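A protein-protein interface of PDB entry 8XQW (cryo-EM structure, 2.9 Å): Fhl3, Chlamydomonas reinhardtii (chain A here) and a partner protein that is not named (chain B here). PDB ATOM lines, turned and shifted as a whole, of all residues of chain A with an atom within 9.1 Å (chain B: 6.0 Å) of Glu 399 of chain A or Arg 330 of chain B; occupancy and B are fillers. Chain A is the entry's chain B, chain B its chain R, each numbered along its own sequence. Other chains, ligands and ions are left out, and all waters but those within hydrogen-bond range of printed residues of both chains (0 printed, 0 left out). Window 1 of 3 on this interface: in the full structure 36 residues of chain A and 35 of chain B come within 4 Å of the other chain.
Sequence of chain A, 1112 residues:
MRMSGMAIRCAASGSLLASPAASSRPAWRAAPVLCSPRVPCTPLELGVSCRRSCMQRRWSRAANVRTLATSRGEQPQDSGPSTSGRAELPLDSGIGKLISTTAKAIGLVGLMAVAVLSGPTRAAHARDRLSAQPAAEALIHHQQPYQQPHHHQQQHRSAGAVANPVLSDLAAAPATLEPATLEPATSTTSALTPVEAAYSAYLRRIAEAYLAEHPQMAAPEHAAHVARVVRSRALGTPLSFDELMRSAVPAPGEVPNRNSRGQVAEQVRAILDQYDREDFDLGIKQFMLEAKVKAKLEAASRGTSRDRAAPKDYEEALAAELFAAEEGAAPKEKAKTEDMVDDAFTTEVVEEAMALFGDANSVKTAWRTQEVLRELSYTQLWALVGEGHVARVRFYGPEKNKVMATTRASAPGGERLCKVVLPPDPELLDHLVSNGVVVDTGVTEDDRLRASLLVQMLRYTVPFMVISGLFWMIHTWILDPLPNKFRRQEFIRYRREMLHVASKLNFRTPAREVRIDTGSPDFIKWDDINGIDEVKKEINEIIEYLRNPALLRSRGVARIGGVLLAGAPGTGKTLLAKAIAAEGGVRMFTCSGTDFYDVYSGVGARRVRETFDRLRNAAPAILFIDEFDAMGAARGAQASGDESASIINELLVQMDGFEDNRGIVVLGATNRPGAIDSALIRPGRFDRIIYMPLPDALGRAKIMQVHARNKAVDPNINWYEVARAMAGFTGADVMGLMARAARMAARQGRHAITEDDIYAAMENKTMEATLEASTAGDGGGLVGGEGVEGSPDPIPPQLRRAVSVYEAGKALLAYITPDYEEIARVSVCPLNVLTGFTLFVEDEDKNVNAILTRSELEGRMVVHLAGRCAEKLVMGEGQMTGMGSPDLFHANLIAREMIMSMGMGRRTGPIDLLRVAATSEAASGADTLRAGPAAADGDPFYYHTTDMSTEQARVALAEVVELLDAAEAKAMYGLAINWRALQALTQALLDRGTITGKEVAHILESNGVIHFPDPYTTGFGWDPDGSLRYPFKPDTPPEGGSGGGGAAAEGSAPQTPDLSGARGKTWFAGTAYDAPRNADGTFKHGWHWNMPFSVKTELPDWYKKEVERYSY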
ATOM      1  N   PHE A 395      23.471  22.649   5.387  1.00  0.00           N
ATOM      2  CA  PHE A 395      23.198  23.423   4.188  1.00  0.00           C
ATOM      3  C   PHE A 395      23.481  22.564   2.971  1.00  0.00           C
ATOM      4  O   PHE A 395      24.536  21.940   2.890  1.00  0.00           O
ATOM      5  CB  PHE A 395      24.065  24.670   4.155  1.00  0.00           C
ATOM      6  CG  PHE A 395      23.685  25.693   5.156  1.00  0.00           C
ATOM      7  CD1 PHE A 395      23.931  25.495   6.485  1.00  0.00           C
ATOM      8  CD2 PHE A 395      23.091  26.858   4.767  1.00  0.00           C
ATOM      9  CE1 PHE A 395      23.590  26.436   7.399  1.00  0.00           C
ATOM     10  CE2 PHE A 395      22.748  27.798   5.679  1.00  0.00           C
ATOM     11  CZ  PHE A 395      22.994  27.586   6.997  1.00  0.00           C
ATOM     12  N   TYR A 396      22.552  22.518   2.029  1.00  0.00           N
ATOM     13  CA  TYR A 396      22.792  21.765   0.816  1.00  0.00           C
ATOM     14  C   TYR A 396      22.247  22.536  -0.371  1.00  0.00           C
ATOM     15  O   TYR A 396      21.664  23.609  -0.229  1.00  0.00           O
ATOM     16  CB  TYR A 396      22.194  20.363   0.902  1.00  0.00           C
ATOM     17  CG  TYR A 396      20.708  20.282   0.712  1.00  0.00           C
ATOM     18  CD1 TYR A 396      19.847  20.409   1.777  1.00  0.00           C
ATOM     19  CD2 TYR A 396      20.167  20.037  -0.528  1.00  0.00           C
ATOM     20  CE1 TYR A 396      18.508  20.325   1.602  1.00  0.00           C
ATOM     21  CE2 TYR A 396      18.830  19.950  -0.702  1.00  0.00           C
ATOM     22  CZ  TYR A 396      18.009  20.099   0.363  1.00  0.00           C
ATOM     23  OH  TYR A 396      16.662  20.010   0.182  1.00  0.00           O
ATOM     24  N   GLY A 397      22.460  21.982  -1.552  1.00  0.00           N
ATOM     25  CA  GLY A 397      22.071  22.632  -2.776  1.00  0.00           C
ATOM     26  C   GLY A 397      23.277  23.191  -3.489  1.00  0.00           C
ATOM     27  O   GLY A 397      24.380  23.230  -2.940  1.00  0.00           O
ATOM     28  N   PRO A 398      23.103  23.624  -4.734  1.00  0.00           N
ATOM     29  CA  PRO A 398      24.224  24.258  -5.433  1.00  0.00           C
ATOM     30  C   PRO A 398      24.456  25.696  -5.010  1.00  0.00           C
ATOM     31  O   PRO A 398      25.569  26.202  -5.179  1.00  0.00           O
ATOM     32  CB  PRO A 398      23.812  24.157  -6.903  1.00  0.00           C
ATOM     33  CG  PRO A 398      22.335  24.152  -6.864  1.00  0.00           C
ATOM     34  CD  PRO A 398      21.932  23.454  -5.608  1.00  0.00           C
ATOM     35  N   GLU A 399      23.446  26.375  -4.469  1.00  0.00           N
ATOM     36  CA  GLU A 399      23.611  27.736  -3.984  1.00  0.00           C
ATOM     37  C   GLU A 399      23.332  27.863  -2.495  1.00  0.00           C
ATOM     38  O   GLU A 399      23.294  28.979  -1.979  1.00  0.00           O
ATOM     39  CB  GLU A 399      22.726  28.700  -4.771  1.00  0.00           C
ATOM     40  CG  GLU A 399      21.261  28.505  -4.564  1.00  0.00           C
ATOM     41  CD  GLU A 399      20.669  27.496  -5.521  1.00  0.00           C
ATOM     42  OE1 GLU A 399      20.193  27.906  -6.599  1.00  0.00           O
ATOM     43  OE2 GLU A 399      20.659  26.292  -5.192  1.00  0.00           O
ATOM     44  N   LYS A 400      23.121  26.754  -1.798  1.00  0.00           N
ATOM     45  CA  LYS A 400      23.227  26.697  -0.345  1.00  0.00           C
ATOM     46  C   LYS A 400      22.209  27.583   0.350  1.00  0.00           C
ATOM     47  O   LYS A 400      22.560  28.389   1.206  1.00  0.00           O
ATOM     48  CB  LYS A 400      24.632  27.073   0.111  1.00  0.00           C
ATOM     49  CG  LYS A 400      25.697  26.118  -0.339  1.00  0.00           C
ATOM     50  CD  LYS A 400      25.941  25.062   0.688  1.00  0.00           C
ATOM     51  CE  LYS A 400      26.931  24.075   0.177  1.00  0.00           C
ATOM     52  NZ  LYS A 400      26.653  23.799  -1.239  1.00  0.00           N
ATOM     53  N   ASN A 401      20.935  27.428   0.010  1.00  0.00           N
ATOM     54  CA  ASN A 401      19.887  28.124   0.736  1.00  0.00           C
ATOM     55  C   ASN A 401      18.836  27.192   1.311  1.00  0.00           C
ATOM     56  O   ASN A 401      17.904  27.664   1.956  1.00  0.00           O
ATOM     57  CB  ASN A 401      19.228  29.176  -0.148  1.00  0.00           C
ATOM     58  CG  ASN A 401      18.635  28.598  -1.383  1.00  0.00           C
ATOM     59  OD1 ASN A 401      18.920  27.470  -1.750  1.00  0.00           O
ATOM     60  ND2 ASN A 401      17.797  29.368  -2.045  1.00  0.00           N
ATOM     61  N   LYS A 402      18.962  25.890   1.107  1.00  0.00           N
ATOM     62  CA  LYS A 402      18.113  24.919   1.767  1.00  0.00           C
ATOM     63  C   LYS A 402      18.899  24.285   2.893  1.00  0.00           C
ATOM     64  O   LYS A 402      20.115  24.153   2.807  1.00  0.00           O
ATOM     65  CB  LYS A 402      17.655  23.836   0.812  1.00  0.00           C
ATOM     66  CG  LYS A 402      16.515  24.221  -0.063  1.00  0.00           C
ATOM     67  CD  LYS A 402      16.950  24.267  -1.494  1.00  0.00           C
ATOM     68  CE  LYS A 402      17.406  22.919  -1.961  1.00  0.00           C
ATOM     69  NZ  LYS A 402      17.723  22.943  -3.408  1.00  0.00           N
ATOM     70  N   VAL A 421      13.568  25.981   3.426  1.00  0.00           N
ATOM     71  CA  VAL A 421      14.130  26.906   2.451  1.00  0.00           C
ATOM     72  C   VAL A 421      14.270  28.260   3.122  1.00  0.00           C
ATOM     73  O   VAL A 421      13.375  28.688   3.852  1.00  0.00           O
ATOM     74  CB  VAL A 421      13.253  26.993   1.197  1.00  0.00           C
ATOM     75  CG1 VAL A 421      14.020  27.580   0.064  1.00  0.00           C
ATOM     76  CG2 VAL A 421      12.758  25.628   0.828  1.00  0.00           C
ATOM     77  N   LEU A 422      15.373  28.926   2.889  1.00  0.00           N
ATOM     78  CA  LEU A 422      15.691  30.037   3.754  1.00  0.00           C
ATOM     79  C   LEU A 422      15.616  31.363   3.024  1.00  0.00           C
ATOM     80  O   LEU A 422      16.076  31.470   1.887  1.00  0.00           O
ATOM     81  CB  LEU A 422      17.095  29.883   4.328  1.00  0.00           C
ATOM     82  CG  LEU A 422      17.373  28.651   5.166  1.00  0.00           C
ATOM     83  CD1 LEU A 422      18.799  28.680   5.585  1.00  0.00           C
ATOM     84  CD2 LEU A 422      16.475  28.648   6.366  1.00  0.00           C
ATOM     85  N   THR A 441      28.116  22.846   6.464  1.00  0.00           N
ATOM     86  CA  THR A 441      28.023  23.363   5.113  1.00  0.00           C
ATOM     87  C   THR A 441      28.508  22.287   4.144  1.00  0.00           C
ATOM     88  O   THR A 441      28.729  21.139   4.524  1.00  0.00           O
ATOM     89  CB  THR A 441      28.814  24.663   5.000  1.00  0.00           C
ATOM     90  OG1 THR A 441      28.776  25.341   6.259  1.00  0.00           O
ATOM     91  CG2 THR A 441      28.190  25.562   3.973  1.00  0.00           C
ATOM     92  N   THR A 444      31.226  23.426  -1.820  1.00  0.00           N
ATOM     93  CA  THR A 444      31.199  24.722  -2.534  1.00  0.00           C
ATOM     94  C   THR A 444      32.416  24.886  -3.417  1.00  0.00           C
ATOM     95  O   THR A 444      33.423  25.436  -2.946  1.00  0.00           O
ATOM     96  CB  THR A 444      31.073  25.870  -1.538  1.00  0.00           C
ATOM     97  OG1 THR A 444      30.259  25.386  -0.475  1.00  0.00           O
ATOM     98  CG2 THR A 444      30.430  27.095  -2.159  1.00  0.00           C
ATOM     99  N   GLU A 445      32.314  24.488  -4.681  1.00  0.00           N
ATOM    100  CA  GLU A 445      33.425  24.693  -5.641  1.00  0.00           C
ATOM    101  C   GLU A 445      33.480  26.179  -6.014  1.00  0.00           C
ATOM    102  O   GLU A 445      32.415  26.819  -6.010  1.00  0.00           O
ATOM    103  CB  GLU A 445      33.174  23.763  -6.821  1.00  0.00           C
ATOM    104  CG  GLU A 445      32.744  22.366  -6.385  1.00  0.00           C
ATOM    105  CD  GLU A 445      33.849  21.501  -5.803  1.00  0.00           C
ATOM    106  OE1 GLU A 445      35.037  21.809  -6.039  1.00  0.00           O
ATOM    107  OE2 GLU A 445      33.525  20.505  -5.126  1.00  0.00           O
ATOM    108  N   ARG A 448      32.168  27.534 -10.540  1.00  0.00           N
ATOM    109  CA  ARG A 448      30.758  27.864 -10.854  1.00  0.00           C
ATOM    110  C   ARG A 448      30.527  27.602 -12.348  1.00  0.00           C
ATOM    111  O   ARG A 448      29.420  27.167 -12.676  1.00  0.00           O
ATOM    112  CB  ARG A 448      30.324  29.258 -10.392  1.00  0.00           C
ATOM    113  CG  ARG A 448      29.288  29.222  -9.281  1.00  0.00           C
ATOM    114  CD  ARG A 448      28.374  30.431  -9.333  1.00  0.00           C
ATOM    115  NE  ARG A 448      27.132  30.194  -8.591  1.00  0.00           N
ATOM    116  CZ  ARG A 448      25.947  30.663  -8.951  1.00  0.00           C
ATOM    117  NH1 ARG A 448      24.884  29.879  -8.924  1.00  0.00           N
ATOM    118  NH2 ARG A 448      25.833  31.919  -9.334  1.00  0.00           N
ATOM    119  N   GLN A 456      25.153  20.330 -16.821  1.00  0.00           N
ATOM    120  CA  GLN A 456      24.178  21.038 -17.643  1.00  0.00           C
ATOM    121  C   GLN A 456      24.043  20.399 -19.016  1.00  0.00           C
ATOM    122  O   GLN A 456      22.931  20.292 -19.553  1.00  0.00           O
ATOM    123  CB  GLN A 456      24.566  22.501 -17.768  1.00  0.00           C
ATOM    124  CG  GLN A 456      24.227  23.301 -16.545  1.00  0.00           C
ATOM    125  CD  GLN A 456      22.774  23.672 -16.472  1.00  0.00           C
ATOM    126  OE1 GLN A 456      22.161  24.008 -17.477  1.00  0.00           O
ATOM    127  NE2 GLN A 456      22.213  23.621 -15.276  1.00  0.00           N
ATOM    128  N   ARG A 459      21.689  17.720 -18.410  1.00  0.00           N
ATOM    129  CA  ARG A 459      20.321  18.205 -18.261  1.00  0.00           C
ATOM    130  C   ARG A 459      19.676  18.477 -19.600  1.00  0.00           C
ATOM    131  O   ARG A 459      18.459  18.357 -19.736  1.00  0.00           O
ATOM    132  CB  ARG A 459      20.289  19.468 -17.419  1.00  0.00           C
ATOM    133  CG  ARG A 459      20.501  19.216 -15.965  1.00  0.00           C
ATOM    134  CD  ARG A 459      20.319  20.475 -15.176  1.00  0.00           C
ATOM    135  NE  ARG A 459      19.147  20.398 -14.323  1.00  0.00           N
ATOM    136  CZ  ARG A 459      17.992  20.986 -14.596  1.00  0.00           C
ATOM    137  NH1 ARG A 459      17.862  21.706 -15.698  1.00  0.00           N
ATOM    138  NH2 ARG A 459      16.974  20.862 -13.764  1.00  0.00           N
ATOM    139  N   ASP B 290      11.167  28.957 -11.922  1.00  0.00           N
ATOM    140  CA  ASP B 290      11.713  30.301 -11.803  1.00  0.00           C
ATOM    141  C   ASP B 290      11.538  31.002 -13.142  1.00  0.00           C
ATOM    142  O   ASP B 290      12.424  31.726 -13.601  1.00  0.00           O
ATOM    143  CB  ASP B 290      13.179  30.241 -11.364  1.00  0.00           C
ATOM    144  CG  ASP B 290      13.775  31.613 -11.060  1.00  0.00           C
ATOM    145  OD1 ASP B 290      13.062  32.628 -11.181  1.00  0.00           O
ATOM    146  OD2 ASP B 290      14.967  31.672 -10.688  1.00  0.00           O
ATOM    147  N   GLY B 327      23.476  27.732 -16.118  1.00  0.00           N
ATOM    148  CA  GLY B 327      22.867  27.529 -14.824  1.00  0.00           C
ATOM    149  C   GLY B 327      23.480  28.376 -13.737  1.00  0.00           C
ATOM    150  O   GLY B 327      23.852  27.861 -12.684  1.00  0.00           O
ATOM    151  N   LEU B 328      23.589  29.677 -13.976  1.00  0.00           N
ATOM    152  CA  LEU B 328      24.141  30.615 -13.010  1.00  0.00           C
ATOM    153  C   LEU B 328      23.151  31.724 -12.692  1.00  0.00           C
ATOM    154  O   LEU B 328      23.549  32.836 -12.355  1.00  0.00           O
ATOM    155  CB  LEU B 328      25.442  31.222 -13.517  1.00  0.00           C
ATOM    156  CG  LEU B 328      26.429  30.318 -14.227  1.00  0.00           C
ATOM    157  CD1 LEU B 328      27.363  31.158 -15.044  1.00  0.00           C
ATOM    158  CD2 LEU B 328      27.189  29.528 -13.210  1.00  0.00           C
ATOM    159  N   GLU B 329      21.859  31.444 -12.801  1.00  0.00           N
ATOM    160  CA  GLU B 329      20.888  32.514 -12.629  1.00  0.00           C
ATOM    161  C   GLU B 329      20.407  32.610 -11.190  1.00  0.00           C
ATOM    162  O   GLU B 329      19.485  33.375 -10.894  1.00  0.00           O
ATOM    163  CB  GLU B 329      19.712  32.315 -13.578  1.00  0.00           C
ATOM    164  CG  GLU B 329      18.794  31.173 -13.207  1.00  0.00           C
ATOM    165  CD  GLU B 329      19.358  29.817 -13.556  1.00  0.00           C
ATOM    166  OE1 GLU B 329      20.221  29.325 -12.802  1.00  0.00           O
ATOM    167  OE2 GLU B 329      18.925  29.234 -14.570  1.00  0.00           O
ATOM    168  N   ARG B 330      20.982  31.860 -10.312  1.00  0.00           N
ATOM    169  CA  ARG B 330      20.619  32.114  -8.932  1.00  0.00           C
ATOM    170  C   ARG B 330      21.851  32.455  -8.102  1.00  0.00           C
ATOM    171  O   ARG B 330      22.930  31.902  -8.317  1.00  0.00           O
ATOM    172  CB  ARG B 330      19.896  30.909  -8.342  1.00  0.00           C
ATOM    173  CG  ARG B 330      18.438  30.913  -8.715  1.00  0.00           C
ATOM    174  CD  ARG B 330      17.702  29.713  -8.181  1.00  0.00           C
ATOM    175  NE  ARG B 330      16.722  29.240  -9.149  1.00  0.00           N
ATOM    176  CZ  ARG B 330      17.006  28.395 -10.131  1.00  0.00           C
ATOM    177  NH1 ARG B 330      18.239  27.929 -10.263  1.00  0.00           N
ATOM    178  NH2 ARG B 330      16.062  28.012 -10.978  1.00  0.00           N
ATOM    179  N   PRO B 331      21.705  33.364  -7.155  1.00  0.00           N
ATOM    180  CA  PRO B 331      22.852  34.148  -6.689  1.00  0.00           C
ATOM    181  C   PRO B 331      23.641  33.686  -5.466  1.00  0.00           C
ATOM    182  O   PRO B 331      24.366  34.517  -4.920  1.00  0.00           O
ATOM    183  CB  PRO B 331      22.213  35.511  -6.419  1.00  0.00           C
ATOM    184  CG  PRO B 331      20.860  35.173  -5.965  1.00  0.00           C
ATOM    185  CD  PRO B 331      20.432  33.953  -6.717  1.00  0.00           C
ATOM    186  N   PHE B 332      23.547  32.439  -5.005  1.00  0.00           N
ATOM    187  CA  PHE B 332      24.419  31.998  -3.911  1.00  0.00           C
ATOM    188  C   PHE B 332      24.241  32.734  -2.588  1.00  0.00           C
ATOM    189  O   PHE B 332      24.901  33.744  -2.347  1.00  0.00           O
ATOM    190  CB  PHE B 332      25.900  32.048  -4.266  1.00  0.00           C
ATOM    191  CG  PHE B 332      26.757  31.423  -3.208  1.00  0.00           C
ATOM    192  CD1 PHE B 332      26.825  30.051  -3.092  1.00  0.00           C
ATOM    193  CD2 PHE B 332      27.435  32.197  -2.290  1.00  0.00           C
ATOM    194  CE1 PHE B 332      27.574  29.469  -2.106  1.00  0.00           C
ATOM    195  CE2 PHE B 332      28.183  31.615  -1.300  1.00  0.00           C
ATOM    196  CZ  PHE B 332      28.252  30.253  -1.211  1.00  0.00           C
ATOM    197  N   TRP B 333      23.319  32.262  -1.759  1.00  0.00           N
ATOM    198  CA  TRP B 333      22.845  32.876  -0.524  1.00  0.00           C
ATOM    199  C   TRP B 333      23.826  33.759   0.246  1.00  0.00           C
ATOM    200  O   TRP B 333      23.442  34.839   0.707  1.00  0.00           O
ATOM    201  CB  TRP B 333      22.395  31.753   0.401  1.00  0.00           C
ATOM    202  CG  TRP B 333      21.411  32.151   1.408  1.00  0.00           C
ATOM    203  CD1 TRP B 333      20.203  32.708   1.181  1.00  0.00           C
ATOM    204  CD2 TRP B 333      21.537  32.018   2.818  1.00  0.00           C
ATOM    205  NE1 TRP B 333      19.560  32.941   2.363  1.00  0.00           N
ATOM    206  CE2 TRP B 333      20.361  32.520   3.387  1.00  0.00           C
ATOM    207  CE3 TRP B 333      22.529  31.522   3.656  1.00  0.00           C
ATOM    208  CZ2 TRP B 333      20.155  32.550   4.749  1.00  0.00           C
ATOM    209  CZ3 TRP B 333      22.322  31.552   5.007  1.00  0.00           C
ATOM    210  CH2 TRP B 333      21.145  32.060   5.543  1.00  0.00           C
ATOM    211  N   GLY B 334      25.067  33.319   0.424  1.00  0.00           N
ATOM    212  CA  GLY B 334      26.021  34.126   1.174  1.00  0.00           C
ATOM    213  C   GLY B 334      26.247  35.500   0.571  1.00  0.00           C
ATOM    214  O   GLY B 334      26.402  36.488   1.292  1.00  0.00           O
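Of chain B, only Arg 330 (3.5 Å), Phe 332 (3.8 Å) and Trp 333 (3.3 Å) come within 4 Å of Glu 399 of chain A. Of the printed residues of chain B, Asn 401 of chain A touches Trp 333. Val 421 of chain A touches none of the printed residues of chain B. Printed residues of chain B within 4 Å of Leu 422 of chain A: Trp 333. Of the printed residues of chain B, Arg 448 of chain A touches Leu 328 (3.3 Å) and Arg 330 (2.9 Å). Of the printed residues of chain B, Gln 456 of chain A touches Gly 327. No residue of chain A comes within 4 Å of Glu 329 of chain B. Arg 330 of chain B touches just these residues of chain A: Glu 399 (3.5 Å) and Arg 448 (2.9 Å). No residue of chain A comes within 4 Å of Pro 331 of chain B. Of the printed residues of chain A, Phe 332 of chain B touches Glu 399 (3.8 Å) and Thr 444 (3.7 Å). The nearest residue of chain A that does not touch Arg 330 of chain B is Asn 401 of chain A (6.1 Å). The nearest printed residue of chain B that does not touch Gln 456 of chain A is Leu 328 of chain B (6.3 Å).
OD2 of Asp 290 of chain B is in salt-bridge range of NE of Arg 330 of chain B (3.4 Å). NH1 of Arg 330 of chain B lies within salt-bridge range of OE1 of Glu 329 of chain B, at 3.5 Å. O of Gly 397 of chain A is in hydrogen-bond range of NZ of Lys 400 of chain A, at 2.9 Å. N of Leu 422 of chain A is in hydrogen-bond range of O of Asn 401 of chain A.
O of Arg 330 of chain B sits at hydrogen-bond distance from NH1 of Arg 448 of chain A (2.9 Å). N of Trp 333 of chain B is in hydrogen-bond range of O of Glu 399 of chain A, 3.3 Å away.
Trp 333 of chain B touches Phe 395 of chain A (CZ3 to CE2, 3.8 Å). CD of Arg 330 of chain B touches OE1 of Glu 399 of chain A, 3.5 Å away. CA of Phe 332 of chain B touches O of Glu 399 of chain A, 3.8 Å away. Trp 333 of chain B touches Lys 400 of chain A. Trp 333 of chain B touches Asn 401 of chain A (CD1 to CB, 3.9 Å). Leu 422 of chain A touches Trp 333 of chain B. Thr 444 of chain A touches Phe 332 of chain B. O of Arg 448 of chain A touches CD2 of Leu 328 of chain B, 3.3 Å away. NE2 of Gln 456 of chain A touches CA of Gly 327 of chain B, at 3.99 Å.
Hydrophobic or aromatic side chains of chain A that line the printed part of chain B: Phe 395. Printed residues of chain B that touch a printed residue of chain A: Gly 327, Leu 328, Arg 330, Phe 332 and Trp 333. Among the printed residues, 11 pairs touch across the chains. Among the printed residues, no Asp or Glu carboxylate lies within 4 Å of a Lys or Arg side-chain nitrogen of the other chain.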
